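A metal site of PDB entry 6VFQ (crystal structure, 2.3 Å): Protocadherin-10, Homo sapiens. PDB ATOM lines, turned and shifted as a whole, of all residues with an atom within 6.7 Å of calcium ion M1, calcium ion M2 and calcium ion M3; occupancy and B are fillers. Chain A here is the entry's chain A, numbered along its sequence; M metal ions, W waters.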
ATOM      1  N   GLU A   9      23.358   1.801   1.597  1.00  0.00           N
ATOM      2  CA  GLU A   9      24.697   1.574   2.121  1.00  0.00           C
ATOM      3  C   GLU A   9      25.433   2.900   2.174  1.00  0.00           C
ATOM      4  O   GLU A   9      25.107   3.841   1.456  1.00  0.00           O
ATOM      5  CB  GLU A   9      25.474   0.579   1.249  1.00  0.00           C
ATOM      6  CG  GLU A   9      25.790   1.125  -0.136  1.00  0.00           C
ATOM      7  CD  GLU A   9      26.898   0.350  -0.855  1.00  0.00           C
ATOM      8  OE1 GLU A   9      27.924   0.005  -0.231  1.00  0.00           O
ATOM      9  OE2 GLU A   9      26.723   0.093  -2.063  1.00  0.00           O
ATOM     10  N   GLU A  10      26.405   2.971   3.073  1.00  0.00           N
ATOM     11  CA  GLU A  10      27.287   4.118   3.212  1.00  0.00           C
ATOM     12  C   GLU A  10      26.589   5.355   3.798  1.00  0.00           C
ATOM     13  O   GLU A  10      27.051   6.477   3.590  1.00  0.00           O
ATOM     14  CB  GLU A  10      27.936   4.467   1.866  1.00  0.00           C
ATOM     15  CG  GLU A  10      28.569   3.259   1.142  1.00  0.00           C
ATOM     16  CD  GLU A  10      29.785   2.650   1.839  1.00  0.00           C
ATOM     17  OE1 GLU A  10      30.234   1.557   1.402  1.00  0.00           O
ATOM     18  OE2 GLU A  10      30.319   3.260   2.802  1.00  0.00           O
ATOM     19  N   ILE A  62      27.557   1.223   6.729  1.00  0.00           N
ATOM     20  CA  ILE A  62      27.412  -0.075   6.085  1.00  0.00           C
ATOM     21  C   ILE A  62      28.036  -0.029   4.704  1.00  0.00           C
ATOM     22  O   ILE A  62      27.633   0.785   3.862  1.00  0.00           O
ATOM     23  CB  ILE A  62      25.929  -0.481   6.002  1.00  0.00           C
ATOM     24  CG1 ILE A  62      25.297  -0.476   7.394  1.00  0.00           C
ATOM     25  CG2 ILE A  62      25.816  -1.845   5.339  1.00  0.00           C
ATOM     26  CD1 ILE A  62      23.787  -0.699   7.383  1.00  0.00           C
ATOM     27  N   ASP A  63      29.034  -0.876   4.467  1.00  0.00           N
ATOM     28  CA  ASP A  63      29.561  -1.134   3.122  1.00  0.00           C
ATOM     29  C   ASP A  63      28.949  -2.434   2.634  1.00  0.00           C
ATOM     30  O   ASP A  63      29.283  -3.520   3.128  1.00  0.00           O
ATOM     31  CB  ASP A  63      31.077  -1.218   3.109  1.00  0.00           C
ATOM     32  CG  ASP A  63      31.639  -1.574   1.719  1.00  0.00           C
ATOM     33  OD1 ASP A  63      30.901  -1.462   0.701  1.00  0.00           O
ATOM     34  OD2 ASP A  63      32.824  -1.974   1.645  1.00  0.00           O
ATOM     35  N   ARG A  64      28.005  -2.326   1.709  1.00  0.00           N
ATOM     36  CA  ARG A  64      27.341  -3.515   1.202  1.00  0.00           C
ATOM     37  C   ARG A  64      28.345  -4.477   0.589  1.00  0.00           C
ATOM     38  O   ARG A  64      28.223  -5.697   0.749  1.00  0.00           O
ATOM     39  CB  ARG A  64      26.284  -3.121   0.164  1.00  0.00           C
ATOM     40  CG  ARG A  64      25.271  -4.224  -0.151  1.00  0.00           C
ATOM     41  CD  ARG A  64      24.721  -4.048  -1.550  1.00  0.00           C
ATOM     42  NE  ARG A  64      25.875  -4.120  -2.448  1.00  0.00           N
ATOM     43  CZ  ARG A  64      26.458  -5.245  -2.847  1.00  0.00           C
ATOM     44  NH1 ARG A  64      25.967  -6.424  -2.488  1.00  0.00           N
ATOM     45  NH2 ARG A  64      27.536  -5.180  -3.612  1.00  0.00           N
ATOM     46  N   GLU A  65      29.355  -3.953  -0.124  1.00  0.00           N
ATOM     47  CA  GLU A  65      30.306  -4.846  -0.773  1.00  0.00           C
ATOM     48  C   GLU A  65      31.015  -5.711   0.241  1.00  0.00           C
ATOM     49  O   GLU A  65      31.448  -6.830  -0.071  1.00  0.00           O
ATOM     50  CB  GLU A  65      31.323  -4.062  -1.609  1.00  0.00           C
ATOM     51  CG  GLU A  65      30.774  -3.544  -2.938  1.00  0.00           C
ATOM     52  CD  GLU A  65      29.661  -2.483  -2.822  1.00  0.00           C
ATOM     53  OE1 GLU A  65      28.539  -2.780  -3.287  1.00  0.00           O
ATOM     54  OE2 GLU A  65      29.912  -1.356  -2.303  1.00  0.00           O
ATOM     55  N   GLN A  66      31.123  -5.240   1.481  1.00  0.00           N
ATOM     56  CA  GLN A  66      31.828  -6.003   2.501  1.00  0.00           C
ATOM     57  C   GLN A  66      30.932  -7.051   3.140  1.00  0.00           C
ATOM     58  O   GLN A  66      31.300  -8.229   3.218  1.00  0.00           O
ATOM     59  CB  GLN A  66      32.405  -5.072   3.553  1.00  0.00           C
ATOM     60  CG  GLN A  66      32.990  -5.839   4.722  1.00  0.00           C
ATOM     61  CD  GLN A  66      34.008  -5.024   5.460  1.00  0.00           C
ATOM     62  OE1 GLN A  66      34.667  -4.172   4.883  1.00  0.00           O
ATOM     63  NE2 GLN A  66      34.132  -5.272   6.760  1.00  0.00           N
ATOM     64  N   LEU A  96      20.526  -1.361   0.399  1.00  0.00           N
ATOM     65  CA  LEU A  96      20.511  -1.109  -1.020  1.00  0.00           C
ATOM     66  C   LEU A  96      21.897  -0.709  -1.511  1.00  0.00           C
ATOM     67  O   LEU A  96      22.578   0.104  -0.873  1.00  0.00           O
ATOM     68  CB  LEU A  96      19.530   0.012  -1.343  1.00  0.00           C
ATOM     69  CG  LEU A  96      18.134  -0.200  -0.753  1.00  0.00           C
ATOM     70  CD1 LEU A  96      17.259   1.007  -1.023  1.00  0.00           C
ATOM     71  CD2 LEU A  96      17.516  -1.475  -1.307  1.00  0.00           C
ATOM     72  N   ASP A  97      22.308  -1.283  -2.645  1.00  0.00           N
ATOM     73  CA  ASP A  97      23.609  -0.999  -3.253  1.00  0.00           C
ATOM     74  C   ASP A  97      23.604   0.366  -3.934  1.00  0.00           C
ATOM     75  O   ASP A  97      22.656   0.701  -4.650  1.00  0.00           O
ATOM     76  CB  ASP A  97      23.956  -2.080  -4.280  1.00  0.00           C
ATOM     77  CG  ASP A  97      25.238  -1.782  -5.080  1.00  0.00           C
ATOM     78  OD1 ASP A  97      26.318  -1.515  -4.473  1.00  0.00           O
ATOM     79  OD2 ASP A  97      25.159  -1.850  -6.336  1.00  0.00           O
ATOM     80  N   ILE A  98      24.655   1.144  -3.709  1.00  0.00           N
ATOM     81  CA  ILE A  98      24.916   2.306  -4.557  1.00  0.00           C
ATOM     82  C   ILE A  98      26.126   2.021  -5.456  1.00  0.00           C
ATOM     83  O   ILE A  98      26.873   1.060  -5.251  1.00  0.00           O
ATOM     84  CB  ILE A  98      25.130   3.589  -3.733  1.00  0.00           C
ATOM     85  CG1 ILE A  98      26.300   3.416  -2.776  1.00  0.00           C
ATOM     86  CG2 ILE A  98      23.892   3.942  -2.965  1.00  0.00           C
ATOM     87  CD1 ILE A  98      26.653   4.692  -2.009  1.00  0.00           C
ATOM     88  N   ASN A  99      26.317   2.894  -6.450  1.00  0.00           N
ATOM     89  CA  ASN A  99      27.387   2.749  -7.432  1.00  0.00           C
ATOM     90  C   ASN A  99      28.626   3.499  -6.961  1.00  0.00           C
ATOM     91  O   ASN A  99      29.012   4.531  -7.518  1.00  0.00           O
ATOM     92  CB  ASN A  99      26.957   3.268  -8.795  1.00  0.00           C
ATOM     93  CG  ASN A  99      27.888   2.790  -9.906  1.00  0.00           C
ATOM     94  OD1 ASN A  99      28.436   1.700  -9.819  1.00  0.00           O
ATOM     95  ND2 ASN A  99      28.064   3.595 -10.957  1.00  0.00           N
ATOM     96  N   ASP A 100      29.254   2.957  -5.916  1.00  0.00           N
ATOM     97  CA  ASP A 100      30.482   3.517  -5.356  1.00  0.00           C
ATOM     98  C   ASP A 100      31.741   2.770  -5.800  1.00  0.00           C
ATOM     99  O   ASP A 100      32.801   2.952  -5.190  1.00  0.00           O
ATOM    100  CB  ASP A 100      30.383   3.556  -3.822  1.00  0.00           C
ATOM    101  CG  ASP A 100      29.919   2.245  -3.212  1.00  0.00           C
ATOM    102  OD1 ASP A 100      29.274   1.455  -3.934  1.00  0.00           O
ATOM    103  OD2 ASP A 100      30.165   2.027  -1.992  1.00  0.00           O
ATOM    104  N   ASN A 101      31.680   1.943  -6.857  1.00  0.00           N
ATOM    105  CA  ASN A 101      32.881   1.254  -7.328  1.00  0.00           C
ATOM    106  C   ASN A 101      32.911   1.243  -8.850  1.00  0.00           C
ATOM    107  O   ASN A 101      31.868   0.950  -9.495  1.00  0.00           O
ATOM    108  CB  ASN A 101      32.994  -0.182  -6.824  1.00  0.00           C
ATOM    109  CG  ASN A 101      33.093  -0.249  -5.323  1.00  0.00           C
ATOM    110  OD1 ASN A 101      34.175  -0.250  -4.764  1.00  0.00           O
ATOM    111  ND2 ASN A 101      31.952  -0.282  -4.667  1.00  0.00           N
ATOM    112  N   PRO A 102      34.059   1.537  -9.450  1.00  0.00           N
ATOM    113  CA  PRO A 102      34.183   1.426 -10.894  1.00  0.00           C
ATOM    114  C   PRO A 102      34.474  -0.012 -11.272  1.00  0.00           C
ATOM    115  O   PRO A 102      34.925  -0.817 -10.443  1.00  0.00           O
ATOM    116  CB  PRO A 102      35.377   2.331 -11.209  1.00  0.00           C
ATOM    117  CG  PRO A 102      36.287   2.134  -9.988  1.00  0.00           C
ATOM    118  CD  PRO A 102      35.357   1.819  -8.809  1.00  0.00           C
ATOM    119  N   PRO A 103      34.246  -0.394 -12.521  1.00  0.00           N
ATOM    120  CA  PRO A 103      34.866  -1.620 -13.014  1.00  0.00           C
ATOM    121  C   PRO A 103      36.383  -1.456 -12.978  1.00  0.00           C
ATOM    122  O   PRO A 103      36.915  -0.346 -13.107  1.00  0.00           O
ATOM    123  CB  PRO A 103      34.318  -1.762 -14.430  1.00  0.00           C
ATOM    124  CG  PRO A 103      33.753  -0.435 -14.764  1.00  0.00           C
ATOM    125  CD  PRO A 103      33.368   0.233 -13.512  1.00  0.00           C
ATOM    126  N   ASP A 131      33.559  -5.496 -11.355  1.00  0.00           N
ATOM    127  CA  ASP A 131      32.887  -4.381 -10.682  1.00  0.00           C
ATOM    128  C   ASP A 131      32.192  -4.930  -9.443  1.00  0.00           C
ATOM    129  O   ASP A 131      31.285  -5.766  -9.585  1.00  0.00           O
ATOM    130  CB  ASP A 131      31.879  -3.703 -11.593  1.00  0.00           C
ATOM    131  CG  ASP A 131      31.357  -2.380 -11.025  1.00  0.00           C
ATOM    132  OD1 ASP A 131      31.036  -2.336  -9.818  1.00  0.00           O
ATOM    133  OD2 ASP A 131      31.292  -1.391 -11.788  1.00  0.00           O
ATOM    134  N   PRO A 132      32.586  -4.538  -8.241  1.00  0.00           N
ATOM    135  CA  PRO A 132      32.032  -5.204  -7.042  1.00  0.00           C
ATOM    136  C   PRO A 132      30.584  -4.831  -6.718  1.00  0.00           C
ATOM    137  O   PRO A 132      29.954  -5.551  -5.942  1.00  0.00           O
ATOM    138  CB  PRO A 132      32.979  -4.757  -5.922  1.00  0.00           C
ATOM    139  CG  PRO A 132      33.516  -3.443  -6.397  1.00  0.00           C
ATOM    140  CD  PRO A 132      33.591  -3.526  -7.903  1.00  0.00           C
ATOM    141  N   ASP A 133      30.048  -3.737  -7.256  1.00  0.00           N
ATOM    142  CA  ASP A 133      28.650  -3.402  -7.062  1.00  0.00           C
ATOM    143  C   ASP A 133      27.790  -4.467  -7.724  1.00  0.00           C
ATOM    144  O   ASP A 133      28.303  -5.321  -8.459  1.00  0.00           O
ATOM    145  CB  ASP A 133      28.350  -2.030  -7.656  1.00  0.00           C
ATOM    146  CG  ASP A 133      29.222  -0.957  -7.060  1.00  0.00           C
ATOM    147  OD1 ASP A 133      29.477  -1.000  -5.842  1.00  0.00           O
ATOM    148  OD2 ASP A 133      29.671  -0.089  -7.838  1.00  0.00           O
ATOM    149  N   VAL A 134      26.478  -4.429  -7.478  1.00  0.00           N
ATOM    150  CA  VAL A 134      25.575  -5.471  -7.980  1.00  0.00           C
ATOM    151  C   VAL A 134      24.555  -4.870  -8.932  1.00  0.00           C
ATOM    152  O   VAL A 134      24.392  -3.653  -9.049  1.00  0.00           O
ATOM    153  CB  VAL A 134      24.865  -6.235  -6.849  1.00  0.00           C
ATOM    154  CG1 VAL A 134      25.836  -7.137  -6.130  1.00  0.00           C
ATOM    155  CG2 VAL A 134      24.181  -5.264  -5.842  1.00  0.00           C
ATOM    156  N   THR A 136      22.468  -3.396 -11.869  1.00  0.00           N
ATOM    157  CA  THR A 136      22.760  -2.369 -12.858  1.00  0.00           C
ATOM    158  C   THR A 136      24.029  -1.602 -12.527  1.00  0.00           C
ATOM    159  O   THR A 136      24.625  -0.998 -13.418  1.00  0.00           O
ATOM    160  CB  THR A 136      21.578  -1.399 -12.984  1.00  0.00           C
ATOM    161  OG1 THR A 136      21.747  -0.593 -14.155  1.00  0.00           O
ATOM    162  CG2 THR A 136      21.487  -0.480 -11.783  1.00  0.00           C
ATOM    163  N   ASN A 137      24.452  -1.577 -11.260  1.00  0.00           N
ATOM    164  CA  ASN A 137      25.678  -0.897 -10.881  1.00  0.00           C
ATOM    165  C   ASN A 137      26.933  -1.679 -11.228  1.00  0.00           C
ATOM    166  O   ASN A 137      28.050  -1.157 -11.053  1.00  0.00           O
ATOM    167  CB  ASN A 137      25.648  -0.601  -9.384  1.00  0.00           C
ATOM    168  CG  ASN A 137      24.606   0.417  -9.050  1.00  0.00           C
ATOM    169  OD1 ASN A 137      24.336   1.323  -9.842  1.00  0.00           O
ATOM    170  ND2 ASN A 137      23.998   0.280  -7.870  1.00  0.00           N
ATOM    171  N   SER A 138      26.785  -2.914 -11.678  1.00  0.00           N
ATOM    172  CA  SER A 138      27.923  -3.741 -12.045  1.00  0.00           C
ATOM    173  C   SER A 138      28.315  -3.522 -13.503  1.00  0.00           C
ATOM    174  O   SER A 138      27.745  -2.702 -14.221  1.00  0.00           O
ATOM    175  CB  SER A 138      27.614  -5.207 -11.787  1.00  0.00           C
ATOM    176  OG  SER A 138      28.823  -5.931 -11.578  1.00  0.00           O
ATOM    177  N   LEU A 139      29.311  -4.290 -13.939  1.00  0.00           N
ATOM    178  CA  LEU A 139      29.847  -4.178 -15.281  1.00  0.00           C
ATOM    179  C   LEU A 139      28.755  -4.323 -16.333  1.00  0.00           C
ATOM    180  O   LEU A 139      27.939  -5.240 -16.270  1.00  0.00           O
ATOM    181  CB  LEU A 139      30.918  -5.252 -15.456  1.00  0.00           C
ATOM    182  CG  LEU A 139      31.569  -5.343 -16.828  1.00  0.00           C
ATOM    183  CD1 LEU A 139      32.449  -4.119 -17.067  1.00  0.00           C
ATOM    184  CD2 LEU A 139      32.379  -6.624 -16.858  1.00  0.00           C
ATOM    185  N   ASP A 188      30.213   0.420 -16.120  1.00  0.00           N
ATOM    186  CA  ASP A 188      29.107  -0.229 -15.444  1.00  0.00           C
ATOM    187  C   ASP A 188      27.814   0.420 -15.930  1.00  0.00           C
ATOM    188  O   ASP A 188      27.812   1.184 -16.895  1.00  0.00           O
ATOM    189  CB  ASP A 188      29.286  -0.175 -13.919  1.00  0.00           C
ATOM    190  CG  ASP A 188      29.346   1.254 -13.356  1.00  0.00           C
ATOM    191  OD1 ASP A 188      28.892   2.213 -14.020  1.00  0.00           O
ATOM    192  OD2 ASP A 188      29.824   1.404 -12.212  1.00  0.00           O
ATOM    193  N   GLY A 189      26.697   0.116 -15.268  1.00  0.00           N
ATOM    194  CA  GLY A 189      25.396   0.537 -15.769  1.00  0.00           C
ATOM    195  C   GLY A 189      24.715   1.608 -14.942  1.00  0.00           C
ATOM    196  O   GLY A 189      23.481   1.621 -14.866  1.00  0.00           O
ATOM    197  N   GLY A 190      25.477   2.507 -14.335  1.00  0.00           N
ATOM    198  CA  GLY A 190      24.891   3.555 -13.537  1.00  0.00           C
ATOM    199  C   GLY A 190      24.609   4.827 -14.317  1.00  0.00           C
ATOM    200  O   GLY A 190      25.487   5.691 -14.438  1.00  0.00           O
ATOM    201  N   ARG A 213      30.355   4.714 -13.872  1.00  0.00           N
ATOM    202  CA  ARG A 213      31.784   4.662 -13.594  1.00  0.00           C
ATOM    203  C   ARG A 213      32.492   3.806 -14.635  1.00  0.00           C
ATOM    204  O   ARG A 213      31.890   2.947 -15.291  1.00  0.00           O
ATOM    205  CB  ARG A 213      32.024   4.149 -12.176  1.00  0.00           C
ATOM    206  CG  ARG A 213      31.178   4.913 -11.163  1.00  0.00           C
ATOM    207  CD  ARG A 213      31.482   4.579  -9.703  1.00  0.00           C
ATOM    208  NE  ARG A 213      32.512   5.465  -9.179  1.00  0.00           N
ATOM    209  CZ  ARG A 213      32.294   6.551  -8.458  1.00  0.00           C
ATOM    210  NH1 ARG A 213      31.061   6.907  -8.133  1.00  0.00           N
ATOM    211  NH2 ARG A 213      33.319   7.285  -8.041  1.00  0.00           N
HETATM  212 CA    CA M   1      29.984  -0.092 -10.260  1.00  0.00          CA
HETATM  213 CA    CA M   2      28.126  -0.431  -3.918  1.00  0.00          CA
HETATM  214 CA    CA M   3      30.288   0.204  -0.699  1.00  0.00          CA
HETATM  215  O   HOH W   1      32.507   0.387  -1.614  1.00  0.00           O
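The side-chain carboxylate (OD2) of Asp 97 sits at hydrogen-bond distance from the backbone NH (N) of Val 134 (3.1 Å). OD1 of Asp 100 lies close to ND2 of Asn 101 (3.3 Å). The side-chain carboxylate (OE2) of Glu 65 sits close to the side-chain amide nitrogen (ND2) of Asn 101. The backbone NH (N) of Glu 9 lies within hydrogen-bond range of the backbone carbonyl oxygen (O) of Leu 96. N of Arg 213 sits at hydrogen-bond distance from OD1 of Asp 188 (2.9 Å). The side-chain carboxylate (OD2) of Asp 97 is in hydrogen-bond range of the side-chain amide nitrogen (ND2) of Asn 137, 2.9 Å away. The guanidinium group (NE) of Arg 64 sits close to the side-chain carboxylate (OD1) of Asp 97 (3.3 Å). The side-chain carboxylate (OE1) of Glu 65 sits close to the guanidinium group (NH2) of Arg 64, 2.6 Å away.
Within 4 Å of calcium ion M1: Asn 99, Asn 101, Asp 131, Asp 133, Asn 137 and Asp 188. Along chain A the residues within 4 Å of calcium ion M1 span positions 99 to 188.
Within 4 Å of calcium ion M2: Glu 9, Glu 65, Asp 97, Ile 98, Asp 100, Asn 101 and Asp 133.
Of the 27 residues printed, 5 come within 4 Å of calcium ion M3. The nearest printed residue that does not touch calcium ion M3 is Arg 64 (4.2 Å).
Calcium ion M1 is bound by the backbone carbonyl oxygen (O) of Asn 101 (2.3 Å), the backbone carbonyl oxygen (O) of Asn 137 (2.3 Å), the side-chain carboxylate (OD2) of Asp 131 (2.4 Å), the side-chain amide oxygen (OD1) of Asn 99 (2.4 Å), the side-chain carboxylate (OD2) of Asp 133 (2.4 Å), the side-chain carboxylate (OD2) of Asp 188 (2.5 Å) and the side-chain carboxylate (OD1) of Asp 131 (2.5 Å).
OD1 of Asp 97 is bound to calcium ion M2. OD1 of Asp 100 binds calcium ion M2 (2.2 Å). O of Ile 98 is bound to calcium ion M2, at 2.4 Å. Calcium ion M2 is bound by OE2 of Glu 9, 2.4 Å away. OD1 of Asp 133 binds calcium ion M2 (2.4 Å). Calcium ion M2 is bound by the side-chain carboxylate (OE1) of Glu 65, at 2.5 Å. Calcium ion M2 is bound by OE2 of Glu 65. Calcium ion M2 has seven donor atoms within binding distance.
The side-chain carboxylate (OD2) of Asp 100 is bound to calcium ion M3, 2.2 Å away. The side-chain carboxylate (OD1) of Asp 63 binds calcium ion M3, at 2.3 Å. OE2 of Glu 65 binds calcium ion M3, 2.3 Å away. Calcium ion M3 is bound by water W1, 2.4 Å away. Calcium ion M3 is bound by the side-chain carboxylate (OE1) of Glu 9 (2.4 Å). The side-chain carboxylate (OE1) of Glu 10 binds calcium ion M3 (2.5 Å). Calcium ion M3 has six donor atoms within binding distance.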
